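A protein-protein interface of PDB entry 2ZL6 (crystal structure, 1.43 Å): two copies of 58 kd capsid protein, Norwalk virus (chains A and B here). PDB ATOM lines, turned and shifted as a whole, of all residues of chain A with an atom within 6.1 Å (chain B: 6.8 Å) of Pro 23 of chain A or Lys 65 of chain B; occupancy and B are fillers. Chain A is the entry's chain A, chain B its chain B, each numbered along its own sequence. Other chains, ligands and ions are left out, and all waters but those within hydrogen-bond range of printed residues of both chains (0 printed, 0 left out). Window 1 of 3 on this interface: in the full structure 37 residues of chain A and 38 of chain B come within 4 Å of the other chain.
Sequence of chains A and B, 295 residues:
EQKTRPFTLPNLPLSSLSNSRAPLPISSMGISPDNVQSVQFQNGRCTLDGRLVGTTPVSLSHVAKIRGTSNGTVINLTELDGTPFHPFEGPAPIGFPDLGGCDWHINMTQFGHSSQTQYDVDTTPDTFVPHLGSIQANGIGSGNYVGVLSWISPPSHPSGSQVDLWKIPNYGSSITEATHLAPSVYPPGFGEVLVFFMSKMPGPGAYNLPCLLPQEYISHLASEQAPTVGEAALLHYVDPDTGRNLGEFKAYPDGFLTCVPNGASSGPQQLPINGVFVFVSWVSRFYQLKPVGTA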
ATOM      1  N   SER A  18       9.524   7.612  21.098  1.00  0.00           N
ATOM      2  CA  SER A  18      10.927   7.250  20.975  1.00  0.00           C
ATOM      3  C   SER A  18      11.764   7.689  22.188  1.00  0.00           C
ATOM      4  O   SER A  18      11.476   8.683  22.842  1.00  0.00           O
ATOM      5  CB  SER A  18      11.566   7.981  19.753  1.00  0.00           C
ATOM      6  OG  SER A  18      12.888   7.585  19.539  1.00  0.00           O
ATOM      7  N   ASN A  19      12.814   6.903  22.428  1.00  0.00           N
ATOM      8  CA  ASN A  19      13.910   7.360  23.281  1.00  0.00           C
ATOM      9  C   ASN A  19      14.466   8.658  22.682  1.00  0.00           C
ATOM     10  O   ASN A  19      14.396   8.854  21.456  1.00  0.00           O
ATOM     11  CB  ASN A  19      15.029   6.330  23.281  1.00  0.00           C
ATOM     12  CG  ASN A  19      15.794   6.321  24.560  1.00  0.00           C
ATOM     13  OD1 ASN A  19      16.658   7.162  24.810  1.00  0.00           O
ATOM     14  ND2 ASN A  19      15.455   5.348  25.421  1.00  0.00           N
ATOM     15  N   ARG A  21      17.740   9.462  23.392  1.00  0.00           N
ATOM     16  CA  ARG A  21      19.189   9.271  23.314  1.00  0.00           C
ATOM     17  C   ARG A  21      19.622   8.365  22.169  1.00  0.00           C
ATOM     18  O   ARG A  21      20.794   8.206  21.884  1.00  0.00           O
ATOM     19  CB  ARG A  21      19.770   8.780  24.657  1.00  0.00           C
ATOM     20  CG  ARG A  21      19.687   9.833  25.733  1.00  0.00           C
ATOM     21  CD  ARG A  21      20.096   9.289  27.110  1.00  0.00           C
ATOM     22  NE  ARG A  21      21.535   9.077  27.204  1.00  0.00           N
ATOM     23  CZ  ARG A  21      22.111   8.229  28.048  1.00  0.00           C
ATOM     24  NH1 ARG A  21      21.364   7.447  28.835  1.00  0.00           N
ATOM     25  NH2 ARG A  21      23.430   8.154  28.096  1.00  0.00           N
ATOM     26  N   ALA A  22      18.635   7.731  21.522  1.00  0.00           N
ATOM     27  CA  ALA A  22      18.872   6.930  20.322  1.00  0.00           C
ATOM     28  C   ALA A  22      17.497   6.727  19.691  1.00  0.00           C
ATOM     29  O   ALA A  22      16.492   6.823  20.380  1.00  0.00           O
ATOM     30  CB  ALA A  22      19.547   5.569  20.650  1.00  0.00           C
ATOM     31  N   PRO A  23      17.461   6.490  18.376  1.00  0.00           N
ATOM     32  CA  PRO A  23      16.163   6.337  17.692  1.00  0.00           C
ATOM     33  C   PRO A  23      15.506   4.968  17.931  1.00  0.00           C
ATOM     34  O   PRO A  23      15.393   4.147  17.000  1.00  0.00           O
ATOM     35  CB  PRO A  23      16.540   6.549  16.214  1.00  0.00           C
ATOM     36  CG  PRO A  23      17.935   6.076  16.115  1.00  0.00           C
ATOM     37  CD  PRO A  23      18.597   6.474  17.427  1.00  0.00           C
ATOM     38  N   LEU A  24      15.023   4.767  19.159  1.00  0.00           N
ATOM     39  CA  LEU A  24      14.490   3.444  19.576  1.00  0.00           C
ATOM     40  C   LEU A  24      13.136   3.597  20.225  1.00  0.00           C
ATOM     41  O   LEU A  24      12.902   4.519  20.995  1.00  0.00           O
ATOM     42  CB  LEU A  24      15.399   2.797  20.635  1.00  0.00           C
ATOM     43  CG  LEU A  24      16.828   2.512  20.184  1.00  0.00           C
ATOM     44  CD1 LEU A  24      17.724   2.201  21.393  1.00  0.00           C
ATOM     45  CD2 LEU A  24      16.933   1.427  19.139  1.00  0.00           C
ATOM     46  N   PRO A  25      12.203   2.662  19.929  1.00  0.00           N
ATOM     47  CA  PRO A  25      10.914   2.725  20.640  1.00  0.00           C
ATOM     48  C   PRO A  25      11.067   2.643  22.162  1.00  0.00           C
ATOM     49  O   PRO A  25      11.961   1.952  22.669  1.00  0.00           O
ATOM     50  CB  PRO A  25      10.177   1.458  20.150  1.00  0.00           C
ATOM     51  CG  PRO A  25      10.809   1.174  18.794  1.00  0.00           C
ATOM     52  CD  PRO A  25      12.270   1.591  18.914  1.00  0.00           C
ATOM     53  N   LEU A  60      14.147  13.709  16.223  1.00  0.00           N
ATOM     54  CA  LEU A  60      14.853  12.437  16.287  1.00  0.00           C
ATOM     55  C   LEU A  60      15.795  12.196  15.103  1.00  0.00           C
ATOM     56  O   LEU A  60      16.721  11.390  15.185  1.00  0.00           O
ATOM     57  CB  LEU A  60      13.833  11.279  16.389  1.00  0.00           C
ATOM     58  CG  LEU A  60      14.432   9.959  16.895  1.00  0.00           C
ATOM     59  CD1 LEU A  60      14.765  10.023  18.383  1.00  0.00           C
ATOM     60  CD2 LEU A  60      13.433   8.845  16.601  1.00  0.00           C
ATOM     61  N   VAL A  63      19.235  12.634  16.343  1.00  0.00           N
ATOM     62  CA  VAL A  63      19.649  12.042  17.631  1.00  0.00           C
ATOM     63  C   VAL A  63      20.648  10.891  17.422  1.00  0.00           C
ATOM     64  O   VAL A  63      20.424   9.988  16.624  1.00  0.00           O
ATOM     65  CB  VAL A  63      18.402  11.568  18.428  1.00  0.00           C
ATOM     66  CG1 VAL A  63      18.811  10.642  19.593  1.00  0.00           C
ATOM     67  CG2 VAL A  63      17.608  12.733  18.951  1.00  0.00           C
ATOM     68  N   ALA A  64      21.761  10.947  18.168  1.00  0.00           N
ATOM     69  CA  ALA A  64      22.823   9.938  18.119  1.00  0.00           C
ATOM     70  C   ALA A  64      23.443   9.824  16.725  1.00  0.00           C
ATOM     71  O   ALA A  64      23.702   8.744  16.204  1.00  0.00           O
ATOM     72  CB  ALA A  64      22.315   8.562  18.629  1.00  0.00           C
ATOM     73  N   VAL A 148      25.185   7.299  12.039  1.00  0.00           N
ATOM     74  CA  VAL A 148      24.157   7.090  13.044  1.00  0.00           C
ATOM     75  C   VAL A 148      24.536   5.897  13.937  1.00  0.00           C
ATOM     76  O   VAL A 148      25.030   4.894  13.465  1.00  0.00           O
ATOM     77  CB  VAL A 148      22.723   6.942  12.413  1.00  0.00           C
ATOM     78  CG1 VAL A 148      22.648   5.754  11.456  1.00  0.00           C
ATOM     79  CG2 VAL A 148      21.659   6.858  13.501  1.00  0.00           C
ATOM     80  N   LEU A 149      24.346   6.045  15.233  1.00  0.00           N
ATOM     81  CA  LEU A 149      24.614   4.924  16.120  1.00  0.00           C
ATOM     82  C   LEU A 149      23.753   3.728  15.731  1.00  0.00           C
ATOM     83  O   LEU A 149      22.541   3.854  15.569  1.00  0.00           O
ATOM     84  CB  LEU A 149      24.309   5.326  17.538  1.00  0.00           C
ATOM     85  CG  LEU A 149      24.672   4.311  18.621  1.00  0.00           C
ATOM     86  CD1 LEU A 149      26.160   4.077  18.717  1.00  0.00           C
ATOM     87  CD2 LEU A 149      24.124   4.858  19.916  1.00  0.00           C
ATOM     88  N   PRO B  23      14.460   8.607   8.315  1.00  0.00           N
ATOM     89  CA  PRO B  23      14.883   9.442   9.442  1.00  0.00           C
ATOM     90  C   PRO B  23      15.963  10.469   9.044  1.00  0.00           C
ATOM     91  O   PRO B  23      17.130  10.365   9.467  1.00  0.00           O
ATOM     92  CB  PRO B  23      15.414   8.383  10.446  1.00  0.00           C
ATOM     93  CG  PRO B  23      15.925   7.271   9.593  1.00  0.00           C
ATOM     94  CD  PRO B  23      14.957   7.222   8.414  1.00  0.00           C
ATOM     95  N   ASN B  43       3.919   6.062   4.062  1.00  0.00           N
ATOM     96  CA  ASN B  43       4.381   6.730   5.280  1.00  0.00           C
ATOM     97  C   ASN B  43       4.202   8.242   5.168  1.00  0.00           C
ATOM     98  O   ASN B  43       4.044   8.782   4.058  1.00  0.00           O
ATOM     99  CB  ASN B  43       5.825   6.349   5.562  1.00  0.00           C
ATOM    100  CG  ASN B  43       5.956   4.909   6.056  1.00  0.00           C
ATOM    101  OD1 ASN B  43       5.045   4.401   6.733  1.00  0.00           O
ATOM    102  ND2 ASN B  43       7.065   4.251   5.687  1.00  0.00           N
ATOM    103  N   LEU B  60       9.177   8.837  14.620  1.00  0.00           N
ATOM    104  CA  LEU B  60      10.254   8.562  13.692  1.00  0.00           C
ATOM    105  C   LEU B  60      11.043   7.302  14.028  1.00  0.00           C
ATOM    106  O   LEU B  60      11.733   6.728  13.164  1.00  0.00           O
ATOM    107  CB  LEU B  60      11.196   9.768  13.612  1.00  0.00           C
ATOM    108  CG  LEU B  60      12.107   9.764  12.400  1.00  0.00           C
ATOM    109  CD1 LEU B  60      11.336  10.109  11.120  1.00  0.00           C
ATOM    110  CD2 LEU B  60      13.217  10.775  12.655  1.00  0.00           C
ATOM    111  N   SER B  61      11.013   6.880  15.302  1.00  0.00           N
ATOM    112  CA  SER B  61      11.737   5.648  15.689  1.00  0.00           C
ATOM    113  C   SER B  61      11.209   4.397  14.995  1.00  0.00           C
ATOM    114  O   SER B  61      11.881   3.362  15.052  1.00  0.00           O
ATOM    115  CB  SER B  61      11.733   5.422  17.214  1.00  0.00           C
ATOM    116  OG  SER B  61      10.418   5.280  17.716  1.00  0.00           O
ATOM    117  N   HIS B  62      10.042   4.506  14.336  1.00  0.00           N
ATOM    118  CA  HIS B  62       9.479   3.379  13.586  1.00  0.00           C
ATOM    119  C   HIS B  62       9.609   3.572  12.067  1.00  0.00           C
ATOM    120  O   HIS B  62       9.230   2.694  11.303  1.00  0.00           O
ATOM    121  CB  HIS B  62       7.983   3.220  13.882  1.00  0.00           C
ATOM    122  CG  HIS B  62       7.641   2.780  15.279  1.00  0.00           C
ATOM    123  ND1 HIS B  62       8.098   3.383  16.440  1.00  0.00           N
ATOM    124  CD2 HIS B  62       6.772   1.820  15.675  1.00  0.00           C
ATOM    125  CE1 HIS B  62       7.556   2.777  17.492  1.00  0.00           C
ATOM    126  NE2 HIS B  62       6.751   1.826  17.049  1.00  0.00           N
ATOM    127  N   VAL B  63      10.095   4.735  11.618  1.00  0.00           N
ATOM    128  CA  VAL B  63      10.024   5.068  10.183  1.00  0.00           C
ATOM    129  C   VAL B  63      11.129   4.417   9.362  1.00  0.00           C
ATOM    130  O   VAL B  63      12.321   4.535   9.673  1.00  0.00           O
ATOM    131  CB  VAL B  63      10.028   6.616   9.993  1.00  0.00           C
ATOM    132  CG1 VAL B  63      10.281   6.998   8.535  1.00  0.00           C
ATOM    133  CG2 VAL B  63       8.702   7.198  10.452  1.00  0.00           C
ATOM    134  N   ALA B  64      10.713   3.759   8.272  1.00  0.00           N
ATOM    135  CA  ALA B  64      11.619   3.069   7.355  1.00  0.00           C
ATOM    136  C   ALA B  64      12.434   1.952   8.025  1.00  0.00           C
ATOM    137  O   ALA B  64      13.629   1.756   7.781  1.00  0.00           O
ATOM    138  CB  ALA B  64      12.543   4.057   6.594  1.00  0.00           C
ATOM    139  N   LYS B  65      11.703   1.198   8.849  1.00  0.00           N
ATOM    140  CA  LYS B  65      12.284   0.078   9.583  1.00  0.00           C
ATOM    141  C   LYS B  65      11.571  -1.216   9.266  1.00  0.00           C
ATOM    142  O   LYS B  65      10.422  -1.219   8.822  1.00  0.00           O
ATOM    143  CB  LYS B  65      12.270   0.319  11.090  1.00  0.00           C
ATOM    144  CG  LYS B  65      13.281   1.374  11.523  1.00  0.00           C
ATOM    145  CD  LYS B  65      13.473   1.365  13.020  1.00  0.00           C
ATOM    146  CE  LYS B  65      14.442   2.466  13.390  1.00  0.00           C
ATOM    147  NZ  LYS B  65      14.572   2.489  14.869  1.00  0.00           N
ATOM    148  N   ILE B  66      12.303  -2.315   9.451  1.00  0.00           N
ATOM    149  CA  ILE B  66      11.710  -3.653   9.315  1.00  0.00           C
ATOM    150  C   ILE B  66      12.082  -4.463  10.545  1.00  0.00           C
ATOM    151  O   ILE B  66      13.091  -4.190  11.213  1.00  0.00           O
ATOM    152  CB  ILE B  66      12.156  -4.385   8.036  1.00  0.00           C
ATOM    153  CG1 ILE B  66      13.627  -4.786   8.104  1.00  0.00           C
ATOM    154  CG2 ILE B  66      11.858  -3.497   6.798  1.00  0.00           C
ATOM    155  CD1 ILE B  66      14.078  -5.658   6.920  1.00  0.00           C
ATOM    156  N   ARG B  67      11.283  -5.497  10.810  1.00  0.00           N
ATOM    157  CA  ARG B  67      11.613  -6.452  11.861  1.00  0.00           C
ATOM    158  C   ARG B  67      11.158  -7.814  11.345  1.00  0.00           C
ATOM    159  O   ARG B  67      10.059  -7.940  10.789  1.00  0.00           O
ATOM    160  CB  ARG B  67      10.886  -6.085  13.142  1.00  0.00           C
ATOM    161  CG  ARG B  67      11.162  -7.035  14.328  1.00  0.00           C
ATOM    162  CD  ARG B  67      12.459  -6.662  15.048  1.00  0.00           C
ATOM    163  NE  ARG B  67      12.858  -7.666  16.051  1.00  0.00           N
ATOM    164  CZ  ARG B  67      12.389  -7.706  17.299  1.00  0.00           C
ATOM    165  NH1 ARG B  67      11.508  -6.813  17.731  1.00  0.00           N
ATOM    166  NH2 ARG B  67      12.808  -8.655  18.136  1.00  0.00           N
ATOM    167  N   LEU B  80       7.379  -3.927  14.377  1.00  0.00           N
ATOM    168  CA  LEU B  80       8.668  -3.577  14.935  1.00  0.00           C
ATOM    169  C   LEU B  80       8.891  -4.187  16.326  1.00  0.00           C
ATOM    170  O   LEU B  80      10.014  -4.569  16.648  1.00  0.00           O
ATOM    171  CB  LEU B  80       8.834  -2.048  14.924  1.00  0.00           C
ATOM    172  CG  LEU B  80      10.154  -1.451  15.413  1.00  0.00           C
ATOM    173  CD1 LEU B  80      11.363  -1.913  14.625  1.00  0.00           C
ATOM    174  CD2 LEU B  80      10.066   0.083  15.354  1.00  0.00           C
ATOM    175  N   PRO B  93       3.926  -4.076   7.414  1.00  0.00           N
ATOM    176  CA  PRO B  93       3.903  -3.655   8.819  1.00  0.00           C
ATOM    177  C   PRO B  93       4.065  -2.127   8.976  1.00  0.00           C
ATOM    178  O   PRO B  93       4.608  -1.470   8.083  1.00  0.00           O
ATOM    179  CB  PRO B  93       5.094  -4.412   9.433  1.00  0.00           C
ATOM    180  CG  PRO B  93       5.296  -5.598   8.535  1.00  0.00           C
ATOM    181  CD  PRO B  93       4.976  -5.073   7.158  1.00  0.00           C
ATOM    182  N   ILE B  94       3.608  -1.596  10.091  1.00  0.00           N
ATOM    183  CA  ILE B  94       3.752  -0.166  10.371  1.00  0.00           C
ATOM    184  C   ILE B  94       5.240   0.232  10.234  1.00  0.00           C
ATOM    185  O   ILE B  94       6.155  -0.491  10.651  1.00  0.00           O
ATOM    186  CB  ILE B  94       3.206   0.172  11.759  1.00  0.00           C
ATOM    187  CG1 ILE B  94       1.693  -0.065  11.795  1.00  0.00           C
ATOM    188  CG2 ILE B  94       3.578   1.618  12.172  1.00  0.00           C
ATOM    189  CD1 ILE B  94       0.870   0.769  10.795  1.00  0.00           C
ATOM    190  N   GLY B  95       5.462   1.362   9.552  1.00  0.00           N
ATOM    191  CA  GLY B  95       6.805   1.914   9.386  1.00  0.00           C
ATOM    192  C   GLY B  95       7.642   1.322   8.262  1.00  0.00           C
ATOM    193  O   GLY B  95       8.748   1.819   7.952  1.00  0.00           O
ATOM    194  N   PHE B  96       7.143   0.252   7.630  1.00  0.00           N
ATOM    195  CA  PHE B  96       7.919  -0.412   6.590  1.00  0.00           C
ATOM    196  C   PHE B  96       8.297   0.614   5.491  1.00  0.00           C
ATOM    197  O   PHE B  96       7.466   1.455   5.174  1.00  0.00           O
ATOM    198  CB  PHE B  96       7.049  -1.548   5.992  1.00  0.00           C
ATOM    199  CG  PHE B  96       7.791  -2.483   5.091  1.00  0.00           C
ATOM    200  CD1 PHE B  96       8.442  -3.607   5.614  1.00  0.00           C
ATOM    201  CD2 PHE B  96       7.787  -2.305   3.703  1.00  0.00           C
ATOM    202  CE1 PHE B  96       9.148  -4.496   4.777  1.00  0.00           C
ATOM    203  CE2 PHE B  96       8.486  -3.195   2.870  1.00  0.00           C
ATOM    204  CZ  PHE B  96       9.163  -4.304   3.421  1.00  0.00           C
ATOM    205  N   PRO B  97       9.530   0.544   4.937  1.00  0.00           N
ATOM    206  CA  PRO B  97       9.883   1.592   3.940  1.00  0.00           C
ATOM    207  C   PRO B  97       8.916   1.629   2.767  1.00  0.00           C
ATOM    208  O   PRO B  97       8.416   0.584   2.333  1.00  0.00           O
ATOM    209  CB  PRO B  97      11.263   1.155   3.445  1.00  0.00           C
ATOM    210  CG  PRO B  97      11.850   0.350   4.625  1.00  0.00           C
ATOM    211  CD  PRO B  97      10.647  -0.400   5.166  1.00  0.00           C
ATOM    212  N   ILE B 106      19.426  -1.758   3.734  1.00  0.00           N
ATOM    213  CA  ILE B 106      18.916  -1.687   5.091  1.00  0.00           C
ATOM    214  C   ILE B 106      19.978  -2.212   6.051  1.00  0.00           C
ATOM    215  O   ILE B 106      20.548  -3.284   5.829  1.00  0.00           O
ATOM    216  CB  ILE B 106      17.615  -2.526   5.170  1.00  0.00           C
ATOM    217  CG1 ILE B 106      16.510  -1.816   4.364  1.00  0.00           C
ATOM    218  CG2 ILE B 106      17.216  -2.805   6.638  1.00  0.00           C
ATOM    219  CD1 ILE B 106      15.151  -2.491   4.364  1.00  0.00           C
ATOM    220  N   VAL B 146      16.368  -6.404  13.509  1.00  0.00           N
ATOM    221  CA  VAL B 146      15.677  -5.142  13.236  1.00  0.00           C
ATOM    222  C   VAL B 146      16.528  -4.455  12.164  1.00  0.00           C
ATOM    223  O   VAL B 146      17.763  -4.539  12.174  1.00  0.00           O
ATOM    224  CB  VAL B 146      15.531  -4.256  14.490  1.00  0.00           C
ATOM    225  CG1 VAL B 146      16.895  -3.931  15.095  1.00  0.00           C
ATOM    226  CG2 VAL B 146      14.730  -2.979  14.180  1.00  0.00           C
ATOM    227  N   GLY B 147      15.857  -3.820  11.202  1.00  0.00           N
ATOM    228  CA  GLY B 147      16.565  -3.134  10.115  1.00  0.00           C
ATOM    229  C   GLY B 147      16.072  -1.717   9.942  1.00  0.00           C
ATOM    230  O   GLY B 147      14.921  -1.436  10.165  1.00  0.00           O
ATOM    231  N   VAL B 148      16.994  -0.822   9.552  1.00  0.00           N
ATOM    232  CA  VAL B 148      16.597   0.571   9.243  1.00  0.00           C
ATOM    233  C   VAL B 148      17.213   0.927   7.896  1.00  0.00           C
ATOM    234  O   VAL B 148      18.376   0.585   7.615  1.00  0.00           O
ATOM    235  CB  VAL B 148      17.034   1.581  10.349  1.00  0.00           C
ATOM    236  CG1 VAL B 148      18.531   1.527  10.587  1.00  0.00           C
ATOM    237  CG2 VAL B 148      16.532   3.016  10.020  1.00  0.00           C
ATOM    238  N   LEU B 149      16.430   1.614   7.066  1.00  0.00           N
ATOM    239  CA  LEU B 149      16.955   2.041   5.774  1.00  0.00           C
ATOM    240  C   LEU B 149      18.165   2.957   5.979  1.00  0.00           C
ATOM    241  O   LEU B 149      18.083   3.908   6.750  1.00  0.00           O
ATOM    242  CB  LEU B 149      15.879   2.767   5.003  1.00  0.00           C
ATOM    243  CG  LEU B 149      16.256   3.301   3.619  1.00  0.00           C
ATOM    244  CD1 LEU B 149      16.585   2.163   2.688  1.00  0.00           C
ATOM    245  CD2 LEU B 149      15.057   4.112   3.108  1.00  0.00           C
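The backbone carbonyl oxygen (O) of Pro 23 of chain A is in hydrogen-bond range of the side-chain amino group (NZ) of Lys 65 of chain B (2.8 Å).
The backbone carbonyl oxygen (O) of Leu 24 of chain A sits close to the side-chain hydroxyl (OG) of Ser 18 of chain A (3.4 Å). The backbone carbonyl oxygen of Leu 24 of chain A lies within hydrogen-bond range of the backbone NH of Asn 19 of chain A (2.8 Å). The side-chain hydroxyl (OG) of Ser 61 of chain B sits at hydrogen-bond distance from a ring nitrogen (ND1) of His 62 of chain B, 3.3 Å away. The side-chain amino group (NZ) of Lys 65 of chain B is in hydrogen-bond range of the backbone carbonyl oxygen (O) of Ser 61 of chain B (2.8 Å). N of Lys 65 of chain B lies within hydrogen-bond range of O of Gly 95 of chain B (3.1 Å). NH1 of Arg 67 of chain B is in hydrogen-bond range of O of Leu 80 of chain B (2.9 Å).
Among the printed residues, merely in contact across the chains: Ser 18 of chain A with Ser 61 of chain B (3.4 Å), Pro 23 of chain A with Ser 61 of chain B (3.9 Å), Leu 24 of chain A with Ser 61 of chain B (3.8 Å), Pro 25 of chain A with Ser 61 of chain B (3.9 Å), Pro 25 of chain A with His 62 of chain B (3.9 Å), Pro 25 of chain A with Leu 80 of chain B (3.7 Å), Leu 60 of chain A with Leu 60 of chain B (3.8 Å) and Leu 60 of chain A with Ser 61 of chain B (3.4 Å).
Of the printed residues of chain B, Ser 18 of chain A touches Ser 61 (3.4 Å). Arg 21 of chain A touches none of the printed residues of chain B. Of chain B, only Ser 61 and Lys 65 come within 4 Å of Pro 23 of chain A. Of the printed residues of chain B, Leu 24 of chain A touches Ser 61. Printed residues of chain B within 4 Å of Leu 60 of chain A: Leu 60 and Ser 61. Printed residues of chain A within 4 Å of Leu 60 of chain B: Leu 60 (3.8 Å). Printed residues of chain A within 4 Å of His 62 of chain B: Pro 25 (3.9 Å). Of chain A, only Pro 23 comes within 4 Å of Lys 65 of chain B. The nearest residue of chain A that does not touch Lys 65 of chain B is Pro 25 of chain A (4.7 Å).
Hydrophobic or aromatic side chains of chain A within 4 Å of the printed part of chain B: Pro 25 and Leu 60. Of the 21 printed residues of chain B, 5 touch a printed residue of chain A. Hydrophobic or aromatic side chains of chain B within 4 Å of the printed part of chain A: Leu 60, His 62 and Leu 80.
Leu 60 of chain B touches its own counterpart, Leu 60 of chain A. Of the 9 pairs that touch across the chains among the printed residues, 1 has its exchanged pair printed and touching as well.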
